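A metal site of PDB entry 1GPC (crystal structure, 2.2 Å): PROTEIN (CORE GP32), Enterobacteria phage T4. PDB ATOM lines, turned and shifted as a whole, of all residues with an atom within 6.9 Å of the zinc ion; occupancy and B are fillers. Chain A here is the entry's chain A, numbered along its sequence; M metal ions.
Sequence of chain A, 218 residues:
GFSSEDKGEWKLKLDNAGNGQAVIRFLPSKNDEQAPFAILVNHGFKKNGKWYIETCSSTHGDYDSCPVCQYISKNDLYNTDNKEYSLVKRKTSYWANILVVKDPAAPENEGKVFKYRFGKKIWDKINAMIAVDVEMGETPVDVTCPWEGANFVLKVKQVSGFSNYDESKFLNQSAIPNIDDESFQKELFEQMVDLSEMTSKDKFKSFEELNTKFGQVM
The side-chain sulfur of Cys 66 lies close to the backbone NH of Val 68, at 3.8 Å.
The side-chain sulfur (SG) of Cys 56 lies close to the side-chain hydroxyl (OG) of Ser 58, at 3.3 Å.
N of Cys 56 lies within hydrogen-bond range of O of Val 41, 2.8 Å away.
Along chain A the residues within 4 Å of the zinc ion span positions 43 to 69.
The zinc ion is bound by SG of Cys 66 (2.1 Å), SG of Cys 69 (2.2 Å) and SG of Cys 56 (2.2 Å).
The zinc ion has three donor atoms within binding distance.
Slightly farther from the zinc ion lies a ring nitrogen (NE2) of His 43 (2.7 Å).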
ATOM      1  N   VAL A  41       4.973 -21.422  14.953  1.00  0.00           N
ATOM      2  CA  VAL A  41       5.364 -20.682  13.755  1.00  0.00           C
ATOM      3  C   VAL A  41       5.232 -21.609  12.561  1.00  0.00           C
ATOM      4  O   VAL A  41       5.457 -22.819  12.676  1.00  0.00           O
ATOM      5  CB  VAL A  41       6.865 -20.191  13.859  1.00  0.00           C
ATOM      6  CG1 VAL A  41       7.191 -19.271  12.717  1.00  0.00           C
ATOM      7  CG2 VAL A  41       7.122 -19.481  15.192  1.00  0.00           C
ATOM      8  N   ASN A  42       4.834 -21.042  11.431  1.00  0.00           N
ATOM      9  CA  ASN A  42       4.687 -21.800  10.204  1.00  0.00           C
ATOM     10  C   ASN A  42       4.946 -20.931   8.973  1.00  0.00           C
ATOM     11  O   ASN A  42       5.413 -19.798   9.058  1.00  0.00           O
ATOM     12  CB  ASN A  42       3.298 -22.449  10.106  1.00  0.00           C
ATOM     13  CG  ASN A  42       2.214 -21.505   9.618  1.00  0.00           C
ATOM     14  OD1 ASN A  42       1.867 -20.538  10.303  1.00  0.00           O
ATOM     15  ND2 ASN A  42       1.691 -21.766   8.427  1.00  0.00           N
ATOM     16  N   HIS A  43       4.745 -21.544   7.831  1.00  0.00           N
ATOM     17  CA  HIS A  43       4.911 -20.909   6.543  1.00  0.00           C
ATOM     18  C   HIS A  43       3.680 -21.394   5.784  1.00  0.00           C
ATOM     19  O   HIS A  43       3.406 -22.606   5.790  1.00  0.00           O
ATOM     20  CB  HIS A  43       6.150 -21.490   5.856  1.00  0.00           C
ATOM     21  CG  HIS A  43       7.419 -20.813   6.257  1.00  0.00           C
ATOM     22  ND1 HIS A  43       7.874 -19.684   5.634  1.00  0.00           N
ATOM     23  CD2 HIS A  43       8.273 -21.060   7.278  1.00  0.00           C
ATOM     24  CE1 HIS A  43       8.950 -19.244   6.248  1.00  0.00           C
ATOM     25  NE2 HIS A  43       9.208 -20.053   7.267  1.00  0.00           N
ATOM     26  N   TYR A  52       2.393 -24.516  -0.011  1.00  0.00           N
ATOM     27  CA  TYR A  52       3.406 -24.925   0.958  1.00  0.00           C
ATOM     28  C   TYR A  52       2.860 -24.390   2.270  1.00  0.00           C
ATOM     29  O   TYR A  52       2.754 -23.192   2.480  1.00  0.00           O
ATOM     30  CB  TYR A  52       4.762 -24.289   0.686  1.00  0.00           C
ATOM     31  CG  TYR A  52       5.778 -24.716   1.716  1.00  0.00           C
ATOM     32  CD1 TYR A  52       5.839 -24.097   2.963  1.00  0.00           C
ATOM     33  CD2 TYR A  52       6.633 -25.783   1.466  1.00  0.00           C
ATOM     34  CE1 TYR A  52       6.714 -24.524   3.925  1.00  0.00           C
ATOM     35  CE2 TYR A  52       7.522 -26.224   2.426  1.00  0.00           C
ATOM     36  CZ  TYR A  52       7.561 -25.598   3.667  1.00  0.00           C
ATOM     37  OH  TYR A  52       8.443 -26.046   4.629  1.00  0.00           O
ATOM     38  N   THR A  55       4.868 -26.433   9.438  1.00  0.00           N
ATOM     39  CA  THR A  55       5.307 -25.815  10.672  1.00  0.00           C
ATOM     40  C   THR A  55       6.765 -25.397  10.492  1.00  0.00           C
ATOM     41  O   THR A  55       7.464 -25.911   9.610  1.00  0.00           O
ATOM     42  CB  THR A  55       5.202 -26.780  11.860  1.00  0.00           C
ATOM     43  OG1 THR A  55       5.976 -27.951  11.606  1.00  0.00           O
ATOM     44  CG2 THR A  55       3.753 -27.168  12.088  1.00  0.00           C
ATOM     45  N   CYS A  56       7.215 -24.455  11.317  1.00  0.00           N
ATOM     46  CA  CYS A  56       8.597 -24.002  11.271  1.00  0.00           C
ATOM     47  C   CYS A  56       9.324 -24.308  12.569  1.00  0.00           C
ATOM     48  O   CYS A  56       8.757 -24.164  13.654  1.00  0.00           O
ATOM     49  CB  CYS A  56       8.643 -22.505  11.019  1.00  0.00           C
ATOM     50  SG  CYS A  56      10.315 -21.937  10.808  1.00  0.00           S
ATOM     51  N   SER A  57      10.574 -24.718  12.473  1.00  0.00           N
ATOM     52  CA  SER A  57      11.356 -25.028  13.670  1.00  0.00           C
ATOM     53  C   SER A  57      11.945 -23.797  14.340  1.00  0.00           C
ATOM     54  O   SER A  57      12.490 -23.874  15.417  1.00  0.00           O
ATOM     55  CB  SER A  57      12.437 -26.052  13.349  1.00  0.00           C
ATOM     56  OG  SER A  57      12.944 -25.864  12.029  1.00  0.00           O
ATOM     57  N   SER A  58      11.818 -22.637  13.703  1.00  0.00           N
ATOM     58  CA  SER A  58      12.289 -21.413  14.312  1.00  0.00           C
ATOM     59  C   SER A  58      11.498 -21.285  15.598  1.00  0.00           C
ATOM     60  O   SER A  58      11.901 -20.593  16.521  1.00  0.00           O
ATOM     61  CB  SER A  58      11.996 -20.224  13.408  1.00  0.00           C
ATOM     62  OG  SER A  58      10.621 -19.929  13.377  1.00  0.00           O
ATOM     63  N   ASP A  62      15.464 -23.280  16.202  1.00  0.00           N
ATOM     64  CA  ASP A  62      16.069 -23.977  15.089  1.00  0.00           C
ATOM     65  C   ASP A  62      15.636 -23.454  13.713  1.00  0.00           C
ATOM     66  O   ASP A  62      14.785 -24.050  13.056  1.00  0.00           O
ATOM     67  CB  ASP A  62      15.764 -25.467  15.212  1.00  0.00           C
ATOM     68  CG  ASP A  62      16.669 -26.316  14.367  1.00  0.00           C
ATOM     69  OD1 ASP A  62      17.511 -25.760  13.617  1.00  0.00           O
ATOM     70  OD2 ASP A  62      16.548 -27.548  14.480  1.00  0.00           O
ATOM     71  N   TYR A  63      16.213 -22.357  13.264  1.00  0.00           N
ATOM     72  CA  TYR A  63      15.863 -21.805  11.954  1.00  0.00           C
ATOM     73  C   TYR A  63      16.485 -22.618  10.791  1.00  0.00           C
ATOM     74  O   TYR A  63      15.904 -22.754   9.706  1.00  0.00           O
ATOM     75  CB  TYR A  63      16.346 -20.354  11.833  1.00  0.00           C
ATOM     76  CG  TYR A  63      15.513 -19.313  12.557  1.00  0.00           C
ATOM     77  CD1 TYR A  63      15.620 -19.136  13.934  1.00  0.00           C
ATOM     78  CD2 TYR A  63      14.697 -18.460  11.844  1.00  0.00           C
ATOM     79  CE1 TYR A  63      14.924 -18.121  14.585  1.00  0.00           C
ATOM     80  CE2 TYR A  63      13.995 -17.438  12.497  1.00  0.00           C
ATOM     81  CZ  TYR A  63      14.116 -17.275  13.871  1.00  0.00           C
ATOM     82  OH  TYR A  63      13.418 -16.261  14.513  1.00  0.00           O
ATOM     83  N   SER A  65      16.900 -25.856  10.344  1.00  0.00           N
ATOM     84  CA  SER A  65      16.158 -27.040   9.912  1.00  0.00           C
ATOM     85  C   SER A  65      14.930 -26.751   9.054  1.00  0.00           C
ATOM     86  O   SER A  65      14.180 -27.682   8.746  1.00  0.00           O
ATOM     87  CB  SER A  65      15.731 -27.870  11.129  1.00  0.00           C
ATOM     88  OG  SER A  65      16.824 -28.556  11.718  1.00  0.00           O
ATOM     89  N   CYS A  66      14.735 -25.494   8.679  1.00  0.00           N
ATOM     90  CA  CYS A  66      13.597 -25.057   7.862  1.00  0.00           C
ATOM     91  C   CYS A  66      14.039 -24.457   6.519  1.00  0.00           C
ATOM     92  O   CYS A  66      14.537 -23.322   6.487  1.00  0.00           O
ATOM     93  CB  CYS A  66      12.793 -24.021   8.633  1.00  0.00           C
ATOM     94  SG  CYS A  66      11.407 -23.298   7.747  1.00  0.00           S
ATOM     95  N   PRO A  67      13.711 -25.123   5.399  1.00  0.00           N
ATOM     96  CA  PRO A  67      14.034 -24.742   4.023  1.00  0.00           C
ATOM     97  C   PRO A  67      13.631 -23.311   3.666  1.00  0.00           C
ATOM     98  O   PRO A  67      14.332 -22.601   2.945  1.00  0.00           O
ATOM     99  CB  PRO A  67      13.209 -25.720   3.191  1.00  0.00           C
ATOM    100  CG  PRO A  67      13.075 -26.894   4.066  1.00  0.00           C
ATOM    101  CD  PRO A  67      12.789 -26.266   5.382  1.00  0.00           C
ATOM    102  N   VAL A  68      12.474 -22.916   4.143  1.00  0.00           N
ATOM    103  CA  VAL A  68      11.970 -21.601   3.849  1.00  0.00           C
ATOM    104  C   VAL A  68      12.731 -20.559   4.669  1.00  0.00           C
ATOM    105  O   VAL A  68      12.924 -19.426   4.232  1.00  0.00           O
ATOM    106  CB  VAL A  68      10.457 -21.499   4.091  1.00  0.00           C
ATOM    107  CG1 VAL A  68       9.874 -20.423   3.230  1.00  0.00           C
ATOM    108  CG2 VAL A  68       9.806 -22.821   3.790  1.00  0.00           C
ATOM    109  N   CYS A  69      13.194 -20.948   5.862  1.00  0.00           N
ATOM    110  CA  CYS A  69      13.953 -19.991   6.685  1.00  0.00           C
ATOM    111  C   CYS A  69      15.310 -19.731   6.010  1.00  0.00           C
ATOM    112  O   CYS A  69      15.745 -18.576   5.907  1.00  0.00           O
ATOM    113  CB  CYS A  69      14.132 -20.499   8.123  1.00  0.00           C
ATOM    114  SG  CYS A  69      12.718 -20.162   9.214  1.00  0.00           S
ATOM    115  N   GLN A  70      15.925 -20.810   5.486  1.00  0.00           N
ATOM    116  CA  GLN A  70      17.201 -20.748   4.791  1.00  0.00           C
ATOM    117  C   GLN A  70      17.072 -19.900   3.556  1.00  0.00           C
ATOM    118  O   GLN A  70      17.914 -19.071   3.273  1.00  0.00           O
ATOM    119  CB  GLN A  70      17.656 -22.145   4.386  1.00  0.00           C
ATOM    120  CG  GLN A  70      17.925 -23.085   5.529  1.00  0.00           C
ATOM    121  CD  GLN A  70      18.823 -24.243   5.123  1.00  0.00           C
ATOM    122  OE1 GLN A  70      19.252 -24.344   3.978  1.00  0.00           O
ATOM    123  NE2 GLN A  70      19.118 -25.105   6.066  1.00  0.00           N
ATOM    124  N   ILE A  72      14.882 -17.452   2.777  1.00  0.00           N
ATOM    125  CA  ILE A  72      14.772 -16.036   3.103  1.00  0.00           C
ATOM    126  C   ILE A  72      16.110 -15.480   3.547  1.00  0.00           C
ATOM    127  O   ILE A  72      16.458 -14.346   3.185  1.00  0.00           O
ATOM    128  CB  ILE A  72      13.741 -15.769   4.222  1.00  0.00           C
ATOM    129  CG1 ILE A  72      12.424 -16.482   3.962  1.00  0.00           C
ATOM    130  CG2 ILE A  72      13.442 -14.281   4.303  1.00  0.00           C
ATOM    131  CD1 ILE A  72      11.424 -16.355   5.122  1.00  0.00           C
ATOM    132  N   ARG A  90       7.498 -16.382   7.624  1.00  0.00           N
ATOM    133  CA  ARG A  90       6.955 -17.246   8.659  1.00  0.00           C
ATOM    134  C   ARG A  90       5.784 -16.579   9.403  1.00  0.00           C
ATOM    135  O   ARG A  90       5.829 -15.378   9.740  1.00  0.00           O
ATOM    136  CB  ARG A  90       8.043 -17.640   9.645  1.00  0.00           C
ATOM    137  CG  ARG A  90       8.705 -16.453  10.325  1.00  0.00           C
ATOM    138  CD  ARG A  90      10.021 -16.806  11.037  1.00  0.00           C
ATOM    139  NE  ARG A  90       9.825 -17.274  12.416  1.00  0.00           N
ATOM    140  CZ  ARG A  90       9.878 -16.491  13.507  1.00  0.00           C
ATOM    141  NH1 ARG A  90      10.118 -15.190  13.411  1.00  0.00           N
ATOM    142  NH2 ARG A  90       9.695 -17.023  14.713  1.00  0.00           N
HETATM  143 ZN    ZN M   1      10.989 -21.441   8.728  1.00  0.00          ZN
